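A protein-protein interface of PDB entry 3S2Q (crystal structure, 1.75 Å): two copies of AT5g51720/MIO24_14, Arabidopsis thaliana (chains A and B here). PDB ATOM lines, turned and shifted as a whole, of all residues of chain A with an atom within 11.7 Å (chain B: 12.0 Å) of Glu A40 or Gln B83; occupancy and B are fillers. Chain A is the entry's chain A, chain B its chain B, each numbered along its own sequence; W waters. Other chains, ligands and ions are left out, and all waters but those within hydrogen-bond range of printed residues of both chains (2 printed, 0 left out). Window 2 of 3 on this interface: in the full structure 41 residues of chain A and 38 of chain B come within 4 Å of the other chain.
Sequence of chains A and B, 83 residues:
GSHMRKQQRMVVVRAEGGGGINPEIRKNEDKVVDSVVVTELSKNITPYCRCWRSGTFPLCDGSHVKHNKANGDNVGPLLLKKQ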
ATOM      1  N   ASP A  34      23.878  26.933  14.797  1.00  0.00           N
ATOM      2  CA  ASP A  34      24.147  25.811  13.907  1.00  0.00           C
ATOM      3  C   ASP A  34      25.414  26.078  13.150  1.00  0.00           C
ATOM      4  O   ASP A  34      25.746  27.240  12.885  1.00  0.00           O
ATOM      5  CB  ASP A  34      22.990  25.623  12.917  1.00  0.00           C
ATOM      6  CG  ASP A  34      21.711  25.205  13.613  1.00  0.00           C
ATOM      7  OD1 ASP A  34      21.633  24.029  14.008  1.00  0.00           O
ATOM      8  OD2 ASP A  34      20.817  26.060  13.774  1.00  0.00           O
ATOM      9  N   SER A  35      26.127  25.003  12.830  1.00  0.00           N
ATOM     10  CA  SER A  35      27.359  25.087  12.078  1.00  0.00           C
ATOM     11  C   SER A  35      27.249  24.403  10.744  1.00  0.00           C
ATOM     12  O   SER A  35      26.606  23.358  10.628  1.00  0.00           O
ATOM     13  CB  SER A  35      28.482  24.437  12.879  1.00  0.00           C
ATOM     14  OG  SER A  35      28.799  25.268  13.972  1.00  0.00           O
ATOM     15  N   VAL A  36      27.901  24.982   9.736  1.00  0.00           N
ATOM     16  CA  VAL A  36      28.030  24.354   8.432  1.00  0.00           C
ATOM     17  C   VAL A  36      29.480  24.334   7.975  1.00  0.00           C
ATOM     18  O   VAL A  36      30.121  25.385   7.835  1.00  0.00           O
ATOM     19  CB  VAL A  36      27.217  25.095   7.376  1.00  0.00           C
ATOM     20  CG1 VAL A  36      27.364  24.411   6.025  1.00  0.00           C
ATOM     21  CG2 VAL A  36      25.763  25.138   7.793  1.00  0.00           C
ATOM     22  N   VAL A  37      29.988  23.130   7.750  1.00  0.00           N
ATOM     23  CA  VAL A  37      31.304  22.963   7.159  1.00  0.00           C
ATOM     24  C   VAL A  37      31.097  23.061   5.645  1.00  0.00           C
ATOM     25  O   VAL A  37      30.474  22.192   5.026  1.00  0.00           O
ATOM     26  CB  VAL A  37      31.960  21.618   7.560  1.00  0.00           C
ATOM     27  CG1 VAL A  37      33.212  21.428   6.767  1.00  0.00           C
ATOM     28  CG2 VAL A  37      32.247  21.556   9.071  1.00  0.00           C
ATOM     29  N   VAL A  38      31.584  24.151   5.065  1.00  0.00           N
ATOM     30  CA  VAL A  38      31.180  24.554   3.719  1.00  0.00           C
ATOM     31  C   VAL A  38      31.669  23.591   2.644  1.00  0.00           C
ATOM     32  O   VAL A  38      31.053  23.466   1.590  1.00  0.00           O
ATOM     33  CB  VAL A  38      31.568  26.043   3.404  1.00  0.00           C
ATOM     34  CG1 VAL A  38      30.863  27.035   4.394  1.00  0.00           C
ATOM     35  CG2 VAL A  38      33.083  26.249   3.421  1.00  0.00           C
ATOM     36  N   THR A  39      32.758  22.887   2.925  1.00  0.00           N
ATOM     37  CA  THR A  39      33.280  21.903   1.967  1.00  0.00           C
ATOM     38  C   THR A  39      32.353  20.679   1.896  1.00  0.00           C
ATOM     39  O   THR A  39      32.516  19.811   1.023  1.00  0.00           O
ATOM     40  CB  THR A  39      34.711  21.451   2.329  1.00  0.00           C
ATOM     41  OG1 THR A  39      34.724  20.894   3.651  1.00  0.00           O
ATOM     42  CG2 THR A  39      35.682  22.619   2.273  1.00  0.00           C
ATOM     43  N   GLU A  40      31.404  20.585   2.822  1.00  0.00           N
ATOM     44  CA  GLU A  40      30.544  19.413   2.875  1.00  0.00           C
ATOM     45  C   GLU A  40      29.177  19.627   2.207  1.00  0.00           C
ATOM     46  O   GLU A  40      28.340  18.699   2.152  1.00  0.00           O
ATOM     47  CB  GLU A  40      30.450  18.878   4.311  1.00  0.00           C
ATOM     48  CG  GLU A  40      31.728  18.114   4.737  1.00  0.00           C
ATOM     49  CD  GLU A  40      31.850  17.880   6.235  1.00  0.00           C
ATOM     50  OE1 GLU A  40      30.908  18.214   6.980  1.00  0.00           O
ATOM     51  OE2 GLU A  40      32.901  17.339   6.675  1.00  0.00           O
ATOM     52  N   LEU A  41      28.955  20.833   1.681  1.00  0.00           N
ATOM     53  CA  LEU A  41      27.764  21.123   0.880  1.00  0.00           C
ATOM     54  C   LEU A  41      27.605  20.128  -0.277  1.00  0.00           C
ATOM     55  O   LEU A  41      28.573  19.805  -0.946  1.00  0.00           O
ATOM     56  CB  LEU A  41      27.809  22.571   0.372  1.00  0.00           C
ATOM     57  CG  LEU A  41      27.605  23.609   1.479  1.00  0.00           C
ATOM     58  CD1 LEU A  41      27.889  25.025   1.002  1.00  0.00           C
ATOM     59  CD2 LEU A  41      26.188  23.506   2.048  1.00  0.00           C
ATOM     60  N   SER A  42      26.378  19.639  -0.476  1.00  0.00           N
ATOM     61  CA  SER A  42      26.046  18.593  -1.468  1.00  0.00           C
ATOM     62  C   SER A  42      25.739  19.105  -2.854  1.00  0.00           C
ATOM     63  O   SER A  42      25.790  18.356  -3.822  1.00  0.00           O
ATOM     64  CB  SER A  42      24.779  17.847  -1.047  1.00  0.00           C
ATOM     65  OG  SER A  42      25.071  16.861  -0.095  1.00  0.00           O
ATOM     66  N   LYS A  43      25.329  20.358  -2.945  1.00  0.00           N
ATOM     67  CA  LYS A  43      24.881  20.894  -4.226  1.00  0.00           C
ATOM     68  C   LYS A  43      25.295  22.340  -4.426  1.00  0.00           C
ATOM     69  O   LYS A  43      25.882  22.951  -3.518  1.00  0.00           O
ATOM     70  CB  LYS A  43      23.375  20.711  -4.382  1.00  0.00           C
ATOM     71  CG  LYS A  43      22.575  21.297  -3.212  1.00  0.00           C
ATOM     72  CD  LYS A  43      21.156  20.849  -3.245  1.00  0.00           C
ATOM     73  CE  LYS A  43      20.315  21.714  -2.294  1.00  0.00           C
ATOM     74  NZ  LYS A  43      18.903  21.251  -2.281  1.00  0.00           N
ATOM     75  N   ASN A  44      25.041  22.865  -5.627  1.00  0.00           N
ATOM     76  CA  ASN A  44      25.524  24.192  -6.005  1.00  0.00           C
ATOM     77  C   ASN A  44      24.984  25.282  -5.071  1.00  0.00           C
ATOM     78  O   ASN A  44      25.748  26.115  -4.585  1.00  0.00           O
ATOM     79  CB  ASN A  44      25.177  24.525  -7.465  1.00  0.00           C
ATOM     80  CG  ASN A  44      25.803  25.846  -7.926  1.00  0.00           C
ATOM     81  OD1 ASN A  44      25.134  26.699  -8.537  1.00  0.00           O
ATOM     82  ND2 ASN A  44      27.092  26.033  -7.605  1.00  0.00           N
ATOM     83  N   ILE A  45      23.678  25.247  -4.810  1.00  0.00           N
ATOM     84  CA  ILE A  45      23.019  26.288  -3.974  1.00  0.00           C
ATOM     85  C   ILE A  45      22.189  25.628  -2.872  1.00  0.00           C
ATOM     86  O   ILE A  45      21.275  24.832  -3.161  1.00  0.00           O
ATOM     87  CB  ILE A  45      22.126  27.266  -4.819  1.00  0.00           C
ATOM     88  CG1 ILE A  45      22.953  27.968  -5.908  1.00  0.00           C
ATOM     89  CG2 ILE A  45      21.481  28.349  -3.909  1.00  0.00           C
ATOM     90  CD1 ILE A  45      22.113  28.673  -6.957  1.00  0.00           C
ATOM     91  N   THR A  46      22.485  25.974  -1.616  1.00  0.00           N
ATOM     92  CA  THR A  46      21.778  25.392  -0.483  1.00  0.00           C
ATOM     93  C   THR A  46      21.198  26.506   0.378  1.00  0.00           C
ATOM     94  O   THR A  46      21.943  27.340   0.891  1.00  0.00           O
ATOM     95  CB  THR A  46      22.692  24.496   0.358  1.00  0.00           C
ATOM     96  OG1 THR A  46      23.324  23.554  -0.510  1.00  0.00           O
ATOM     97  CG2 THR A  46      21.865  23.725   1.430  1.00  0.00           C
ATOM     98  N   PRO A  47      19.855  26.528   0.535  1.00  0.00           N
ATOM     99  CA  PRO A  47      19.252  27.614   1.336  1.00  0.00           C
ATOM    100  C   PRO A  47      19.147  27.276   2.830  1.00  0.00           C
ATOM    101  O   PRO A  47      18.711  26.162   3.200  1.00  0.00           O
ATOM    102  CB  PRO A  47      17.862  27.795   0.696  1.00  0.00           C
ATOM    103  CG  PRO A  47      17.519  26.387   0.159  1.00  0.00           C
ATOM    104  CD  PRO A  47      18.840  25.628  -0.048  1.00  0.00           C
ATOM    105  N   TYR A  48      19.555  28.233   3.666  1.00  0.00           N
ATOM    106  CA  TYR A  48      19.492  28.094   5.102  1.00  0.00           C
ATOM    107  C   TYR A  48      18.455  29.049   5.648  1.00  0.00           C
ATOM    108  O   TYR A  48      18.345  30.188   5.196  1.00  0.00           O
ATOM    109  CB  TYR A  48      20.881  28.298   5.753  1.00  0.00           C
ATOM    110  CG  TYR A  48      21.666  27.010   5.671  1.00  0.00           C
ATOM    111  CD1 TYR A  48      21.767  26.172   6.781  1.00  0.00           C
ATOM    112  CD2 TYR A  48      22.245  26.589   4.465  1.00  0.00           C
ATOM    113  CE1 TYR A  48      22.427  24.963   6.712  1.00  0.00           C
ATOM    114  CE2 TYR A  48      22.950  25.374   4.391  1.00  0.00           C
ATOM    115  CZ  TYR A  48      23.026  24.574   5.528  1.00  0.00           C
ATOM    116  OH  TYR A  48      23.701  23.378   5.531  1.00  0.00           O
ATOM    117  N   LEU A  59      17.953  24.139   7.688  1.00  0.00           N
ATOM    118  CA  LEU A  59      17.762  24.308   6.251  1.00  0.00           C
ATOM    119  C   LEU A  59      16.442  25.065   6.014  1.00  0.00           C
ATOM    120  O   LEU A  59      15.533  25.026   6.864  1.00  0.00           O
ATOM    121  CB  LEU A  59      17.727  22.951   5.535  1.00  0.00           C
ATOM    122  CG  LEU A  59      19.037  22.144   5.443  1.00  0.00           C
ATOM    123  CD1 LEU A  59      18.775  20.745   4.854  1.00  0.00           C
ATOM    124  CD2 LEU A  59      20.065  22.892   4.605  1.00  0.00           C
ATOM    125  N   LEU A  80      23.831  29.418   0.329  1.00  0.00           N
ATOM    126  CA  LEU A  80      25.249  29.035   0.351  1.00  0.00           C
ATOM    127  C   LEU A  80      25.580  28.444  -1.010  1.00  0.00           C
ATOM    128  O   LEU A  80      24.899  27.513  -1.468  1.00  0.00           O
ATOM    129  CB  LEU A  80      25.527  28.042   1.479  1.00  0.00           C
ATOM    130  CG  LEU A  80      25.227  28.497   2.916  1.00  0.00           C
ATOM    131  CD1 LEU A  80      25.777  27.493   3.889  1.00  0.00           C
ATOM    132  CD2 LEU A  80      25.806  29.881   3.211  1.00  0.00           C
ATOM    133  N   LYS A  81      26.570  29.035  -1.676  1.00  0.00           N
ATOM    134  CA  LYS A  81      26.840  28.723  -3.088  1.00  0.00           C
ATOM    135  C   LYS A  81      28.263  28.200  -3.233  1.00  0.00           C
ATOM    136  O   LYS A  81      29.197  28.753  -2.644  1.00  0.00           O
ATOM    137  CB  LYS A  81      26.658  29.965  -3.960  1.00  0.00           C
ATOM    138  CG  LYS A  81      25.237  30.576  -3.868  1.00  0.00           C
ATOM    139  CD  LYS A  81      25.097  31.777  -4.763  1.00  0.00           C
ATOM    140  CE  LYS A  81      23.613  32.105  -4.902  1.00  0.00           C
ATOM    141  NZ  LYS A  81      23.360  33.279  -5.793  1.00  0.00           N
ATOM    142  N   LYS A  82      28.401  27.124  -4.007  1.00  0.00           N
ATOM    143  CA  LYS A  82      29.693  26.517  -4.285  1.00  0.00           C
ATOM    144  C   LYS A  82      30.417  27.391  -5.296  1.00  0.00           C
ATOM    145  O   LYS A  82      31.622  27.443  -5.316  1.00  0.00           O
ATOM    146  CB  LYS A  82      29.495  25.136  -4.894  1.00  0.00           C
ATOM    147  CG  LYS A  82      29.220  24.058  -3.909  1.00  0.00           C
ATOM    148  CD  LYS A  82      29.450  22.700  -4.586  1.00  0.00           C
ATOM    149  CE  LYS A  82      29.082  21.539  -3.672  1.00  0.00           C
ATOM    150  NZ  LYS A  82      30.219  21.075  -2.841  1.00  0.00           N
ATOM    151  N   VAL B  36      26.238  33.685  -0.372  1.00  0.00           N
ATOM    152  CA  VAL B  36      27.633  33.565   0.092  1.00  0.00           C
ATOM    153  C   VAL B  36      28.248  32.541  -0.824  1.00  0.00           C
ATOM    154  O   VAL B  36      27.808  31.386  -0.854  1.00  0.00           O
ATOM    155  CB  VAL B  36      27.753  33.074   1.560  1.00  0.00           C
ATOM    156  CG1 VAL B  36      29.258  33.009   1.993  1.00  0.00           C
ATOM    157  CG2 VAL B  36      27.024  33.995   2.500  1.00  0.00           C
ATOM    158  N   VAL B  37      29.253  32.969  -1.592  1.00  0.00           N
ATOM    159  CA  VAL B  37      30.034  32.024  -2.392  1.00  0.00           C
ATOM    160  C   VAL B  37      31.059  31.540  -1.380  1.00  0.00           C
ATOM    161  O   VAL B  37      31.871  32.332  -0.909  1.00  0.00           O
ATOM    162  CB  VAL B  37      30.648  32.709  -3.615  1.00  0.00           C
ATOM    163  CG1 VAL B  37      31.649  31.784  -4.331  1.00  0.00           C
ATOM    164  CG2 VAL B  37      29.521  33.174  -4.559  1.00  0.00           C
ATOM    165  N   VAL B  38      30.965  30.275  -0.981  1.00  0.00           N
ATOM    166  CA  VAL B  38      31.656  29.805   0.234  1.00  0.00           C
ATOM    167  C   VAL B  38      33.172  29.794   0.101  1.00  0.00           C
ATOM    168  O   VAL B  38      33.886  29.936   1.112  1.00  0.00           O
ATOM    169  CB  VAL B  38      31.137  28.423   0.726  1.00  0.00           C
ATOM    170  CG1 VAL B  38      29.637  28.517   1.152  1.00  0.00           C
ATOM    171  CG2 VAL B  38      31.401  27.314  -0.315  1.00  0.00           C
ATOM    172  N   THR B  39      33.672  29.658  -1.136  1.00  0.00           N
ATOM    173  CA  THR B  39      35.147  29.661  -1.351  1.00  0.00           C
ATOM    174  C   THR B  39      35.721  31.044  -1.106  1.00  0.00           C
ATOM    175  O   THR B  39      36.942  31.200  -1.015  1.00  0.00           O
ATOM    176  CB  THR B  39      35.541  29.271  -2.783  1.00  0.00           C
ATOM    177  OG1 THR B  39      34.828  30.110  -3.691  1.00  0.00           O
ATOM    178  CG2 THR B  39      35.234  27.801  -3.071  1.00  0.00           C
ATOM    179  N   GLU B  40      34.840  32.044  -0.979  1.00  0.00           N
ATOM    180  CA  GLU B  40      35.250  33.422  -0.739  1.00  0.00           C
ATOM    181  C   GLU B  40      35.421  33.739   0.769  1.00  0.00           C
ATOM    182  O   GLU B  40      35.943  34.804   1.117  1.00  0.00           O
ATOM    183  CB  GLU B  40      34.269  34.424  -1.370  1.00  0.00           C
ATOM    184  CG  GLU B  40      34.196  34.444  -2.913  1.00  0.00           C
ATOM    185  CD  GLU B  40      33.193  35.487  -3.458  1.00  0.00           C
ATOM    186  OE1 GLU B  40      32.548  36.205  -2.666  1.00  0.00           O
ATOM    187  OE2 GLU B  40      33.048  35.607  -4.696  1.00  0.00           O
ATOM    188  N   LEU B  41      34.962  32.856   1.653  1.00  0.00           N
ATOM    189  CA  LEU B  41      35.105  33.089   3.082  1.00  0.00           C
ATOM    190  C   LEU B  41      36.592  33.133   3.380  1.00  0.00           C
ATOM    191  O   LEU B  41      37.364  32.426   2.743  1.00  0.00           O
ATOM    192  CB  LEU B  41      34.450  31.971   3.876  1.00  0.00           C
ATOM    193  CG  LEU B  41      32.934  31.978   3.705  1.00  0.00           C
ATOM    194  CD1 LEU B  41      32.329  30.645   4.111  1.00  0.00           C
ATOM    195  CD2 LEU B  41      32.327  33.113   4.500  1.00  0.00           C
ATOM    196  N   SER B  42      37.002  33.977   4.304  1.00  0.00           N
ATOM    197  CA  SER B  42      38.422  34.010   4.643  1.00  0.00           C
ATOM    198  C   SER B  42      38.748  33.553   6.057  1.00  0.00           C
ATOM    199  O   SER B  42      39.739  32.874   6.262  1.00  0.00           O
ATOM    200  CB  SER B  42      39.029  35.370   4.356  1.00  0.00           C
ATOM    201  OG  SER B  42      38.442  36.348   5.164  1.00  0.00           O
ATOM    202  N   LYS B  43      37.900  33.905   7.025  1.00  0.00           N
ATOM    203  CA  LYS B  43      38.055  33.418   8.399  1.00  0.00           C
ATOM    204  C   LYS B  43      37.673  31.950   8.472  1.00  0.00           C
ATOM    205  O   LYS B  43      36.938  31.446   7.609  1.00  0.00           O
ATOM    206  CB  LYS B  43      37.152  34.202   9.376  1.00  0.00           C
ATOM    207  CG  LYS B  43      37.588  35.642   9.598  1.00  0.00           C
ATOM    208  CD  LYS B  43      36.750  36.290  10.669  1.00  0.00           C
ATOM    209  CE  LYS B  43      35.308  36.450  10.283  1.00  0.00           C
ATOM    210  NZ  LYS B  43      34.782  37.292  11.395  1.00  0.00           N
ATOM    211  N   ASN B  44      38.169  31.257   9.491  1.00  0.00           N
ATOM    212  CA  ASN B  44      37.801  29.860   9.713  1.00  0.00           C
ATOM    213  C   ASN B  44      36.335  29.708  10.113  1.00  0.00           C
ATOM    214  O   ASN B  44      35.655  28.772   9.658  1.00  0.00           O
ATOM    215  CB  ASN B  44      38.707  29.218  10.750  1.00  0.00           C
ATOM    216  CG  ASN B  44      40.117  29.008  10.219  1.00  0.00           C
ATOM    217  OD1 ASN B  44      40.350  29.101   9.002  1.00  0.00           O
ATOM    218  ND2 ASN B  44      41.062  28.736  11.118  1.00  0.00           N
ATOM    219  N   ILE B  45      35.856  30.645  10.931  1.00  0.00           N
ATOM    220  CA  ILE B  45      34.441  30.679  11.297  1.00  0.00           C
ATOM    221  C   ILE B  45      33.870  32.067  11.015  1.00  0.00           C
ATOM    222  O   ILE B  45      34.422  33.076  11.468  1.00  0.00           O
ATOM    223  CB  ILE B  45      34.229  30.276  12.803  1.00  0.00           C
ATOM    224  CG1 ILE B  45      34.895  28.920  13.120  1.00  0.00           C
ATOM    225  CG2 ILE B  45      32.733  30.264  13.164  1.00  0.00           C
ATOM    226  CD1 ILE B  45      35.050  28.655  14.628  1.00  0.00           C
ATOM    227  N   THR B  46      32.758  32.130  10.268  1.00  0.00           N
ATOM    228  CA  THR B  46      32.119  33.419   9.965  1.00  0.00           C
ATOM    229  C   THR B  46      30.657  33.292  10.347  1.00  0.00           C
ATOM    230  O   THR B  46      29.937  32.445   9.778  1.00  0.00           O
ATOM    231  CB  THR B  46      32.255  33.781   8.451  1.00  0.00           C
ATOM    232  OG1 THR B  46      33.629  33.643   8.056  1.00  0.00           O
ATOM    233  CG2 THR B  46      31.792  35.220   8.174  1.00  0.00           C
ATOM    234  N   PRO B  47      30.206  34.104  11.329  1.00  0.00           N
ATOM    235  CA  PRO B  47      28.830  34.002  11.820  1.00  0.00           C
ATOM    236  C   PRO B  47      27.863  34.899  11.014  1.00  0.00           C
ATOM    237  O   PRO B  47      28.151  36.082  10.745  1.00  0.00           O
ATOM    238  CB  PRO B  47      28.947  34.482  13.261  1.00  0.00           C
ATOM    239  CG  PRO B  47      30.009  35.582  13.154  1.00  0.00           C
ATOM    240  CD  PRO B  47      30.975  35.124  12.068  1.00  0.00           C
ATOM    241  N   LEU B  79      26.909  29.419  11.724  1.00  0.00           N
ATOM    242  CA  LEU B  79      28.372  29.519  11.658  1.00  0.00           C
ATOM    243  C   LEU B  79      28.903  28.824  10.394  1.00  0.00           C
ATOM    244  O   LEU B  79      28.789  27.609  10.262  1.00  0.00           O
ATOM    245  CB  LEU B  79      28.999  28.880  12.894  1.00  0.00           C
ATOM    246  CG  LEU B  79      28.562  29.390  14.282  1.00  0.00           C
ATOM    247  CD1 LEU B  79      29.477  28.812  15.383  1.00  0.00           C
ATOM    248  CD2 LEU B  79      28.540  30.914  14.389  1.00  0.00           C
ATOM    249  N   LEU B  80      29.471  29.598   9.474  1.00  0.00           N
ATOM    250  CA  LEU B  80      30.069  29.006   8.268  1.00  0.00           C
ATOM    251  C   LEU B  80      31.523  28.715   8.562  1.00  0.00           C
ATOM    252  O   LEU B  80      32.302  29.614   8.926  1.00  0.00           O
ATOM    253  CB  LEU B  80      29.893  29.917   7.049  1.00  0.00           C
ATOM    254  CG  LEU B  80      28.454  30.405   6.773  1.00  0.00           C
ATOM    255  CD1 LEU B  80      28.436  31.156   5.471  1.00  0.00           C
ATOM    256  CD2 LEU B  80      27.501  29.228   6.691  1.00  0.00           C
ATOM    257  N   LYS B  81      31.888  27.443   8.454  1.00  0.00           N
ATOM    258  CA  LYS B  81      33.227  27.010   8.853  1.00  0.00           C
ATOM    259  C   LYS B  81      33.998  26.475   7.653  1.00  0.00           C
ATOM    260  O   LYS B  81      33.443  25.755   6.823  1.00  0.00           O
ATOM    261  CB  LYS B  81      33.141  25.929   9.937  1.00  0.00           C
ATOM    262  CG  LYS B  81      32.336  26.347  11.133  1.00  0.00           C
ATOM    263  CD  LYS B  81      32.345  25.326  12.244  1.00  0.00           C
ATOM    264  CE  LYS B  81      32.131  26.076  13.551  1.00  0.00           C
ATOM    265  NZ  LYS B  81      32.022  25.237  14.783  1.00  0.00           N
ATOM    266  N   LYS B  82      35.273  26.847   7.556  1.00  0.00           N
ATOM    267  CA  LYS B  82      36.149  26.290   6.508  1.00  0.00           C
ATOM    268  C   LYS B  82      36.518  24.833   6.809  1.00  0.00           C
ATOM    269  O   LYS B  82      36.865  24.067   5.872  1.00  0.00           O
ATOM    270  CB  LYS B  82      37.404  27.154   6.371  1.00  0.00           C
ATOM    271  CG  LYS B  82      37.137  28.434   5.673  1.00  0.00           C
ATOM    272  CD  LYS B  82      38.401  29.253   5.569  1.00  0.00           C
ATOM    273  CE  LYS B  82      38.263  30.315   4.518  1.00  0.00           C
ATOM    274  NZ  LYS B  82      38.549  29.762   3.181  1.00  0.00           N
ATOM    275  N   GLN B  83      36.376  24.479   8.100  1.00  0.00           N
ATOM    276  CA  GLN B  83      36.844  23.260   8.799  1.00  0.00           C
ATOM    277  C   GLN B  83      38.368  23.056   8.753  1.00  0.00           C
ATOM    278  O   GLN B  83      39.127  23.875   9.278  1.00  0.00           O
ATOM    279  CB  GLN B  83      36.133  22.007   8.324  1.00  0.00           C
ATOM    280  CG  GLN B  83      36.372  20.773   9.197  1.00  0.00           C
ATOM    281  CD  GLN B  83      36.166  19.459   8.418  1.00  0.00           C
ATOM    282  OE1 GLN B  83      35.569  18.494   8.932  1.00  0.00           O
ATOM    283  NE2 GLN B  83      36.654  19.422   7.168  1.00  0.00           N
HETATM  284  O   HOH W   1      34.050  29.209  -6.152  1.00  0.00           O
HETATM  285  O   HOH W   2      37.649  21.038   5.137  1.00  0.00           O
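The backbone NH of Leu B79 sits at hydrogen-bond distance from the backbone carbonyl oxygen of Asp A34, 2.7 Å away.
The side-chain hydroxyl (OG) of Ser A35 sits at hydrogen-bond distance from the side-chain amino group (NZ) of Lys B81, 3.3 Å away.
The backbone NH of Val A36 lies within hydrogen-bond range of the backbone carbonyl oxygen of Leu B79 (2.8 Å).
The backbone carbonyl oxygen (O) of Val A36 is in hydrogen-bond range of the backbone NH (N) of Lys B81 (2.8 Å).
The backbone NH (N) of Val A38 lies within hydrogen-bond range of the backbone carbonyl oxygen (O) of Lys B81 (3.0 Å).
The backbone carbonyl oxygen (O) of Val B36 sits at hydrogen-bond distance from the backbone NH (N) of Lys A81, 2.8 Å away.
The backbone NH of Val B38 is in hydrogen-bond range of the backbone carbonyl oxygen of Lys A81 (2.9 Å).
O of Leu A41 lies within hydrogen-bond range of NZ of Lys A82 (2.8 Å).
O of Thr A46 lies within hydrogen-bond range of N of Leu A80 (2.9 Å).
O of Leu B41 lies close to NZ of Lys B82 (2.9 Å).
The backbone NH (N) of Thr B46 sits at hydrogen-bond distance from the backbone carbonyl oxygen (O) of Leu B80 (2.9 Å).
Among the printed residues, merely in contact across the chains: Ser A35 with Leu B79 (3.4 Å), Val A36 with Leu B80 (3.6 Å), Val A37 with Lys B81 (3.5 Å), Val A37 with Gln B83 (3.4 Å), Val A38 with Val B38 (3.6 Å), Val A38 with Leu B41 (3.9 Å), Glu A40 with Gln B83 (3.7 Å), Leu A41 with Val B38 (3.9 Å), Leu A80 with Val B36 (3.7 Å), Leu A80 with Leu B80 (3.7 Å) and Lys A81 with Val B37 (3.4 Å).
Gln B83 touches two residues of chain A.
Of the printed residues of chain B, Val A37 touches Lys B81 and Gln B83.
Val A38 touches three residues of chain B.
No residue of chain B comes within 4 Å of Thr A39.
No residue of chain B comes within 4 Å of Ser A42.
No residue of chain A comes within 4 Å of Asn B44.
No residue of chain A comes within 4 Å of Lys B82.
Of the printed residues of chain A, Leu B41 touches Val A38.
Of the printed residues of chain A, Leu B80 touches Val A36 (3.6 Å) and Leu A80 (3.7 Å).
Lys B43 touches none of the printed residues of chain A.
The nearest residue of chain A that does not touch Gln B83 is Thr A39 (4.3 Å).
Of the 17 printed residues of chain B, 8 touch a printed residue of chain A.
Hydrophobic or aromatic side chains of chain B that line the printed part of chain A: Val B38, Leu B41, Leu B79 and Leu B80.
Of the 19 printed residues of chain A, 9 touch a printed residue of chain B.
Hydrophobic or aromatic side chains of chain A that line the printed part of chain B: Val A37, Val A38, Leu A41 and Leu A80.
Among the printed residues, no Asp or Glu carboxylate lies within 4 Å of a Lys or Arg side-chain nitrogen of the other chain.
Val A36 touches Leu B80, and with the chains exchanged Leu A80 touches Val B36.
Val A37 touches Lys B81, and with the chains exchanged Lys A81 touches Val B37.
Val A38 touches Lys B81, and with the chains exchanged Lys A81 touches Val B38.
Leu B80 touches its own counterpart, Leu A80.
Positions printed for both chains: 36, 37, 38, 39, 40, 41, 42, 43, 44, 45, 46, 47, 80, 81 and 82.
Water W1 bridges OG1 of Thr B39 and O of Lys A82.
Water W2 lies within hydrogen-bond range of NE2 of Gln B83, O of Lys B82 and OG1 of Thr A39.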
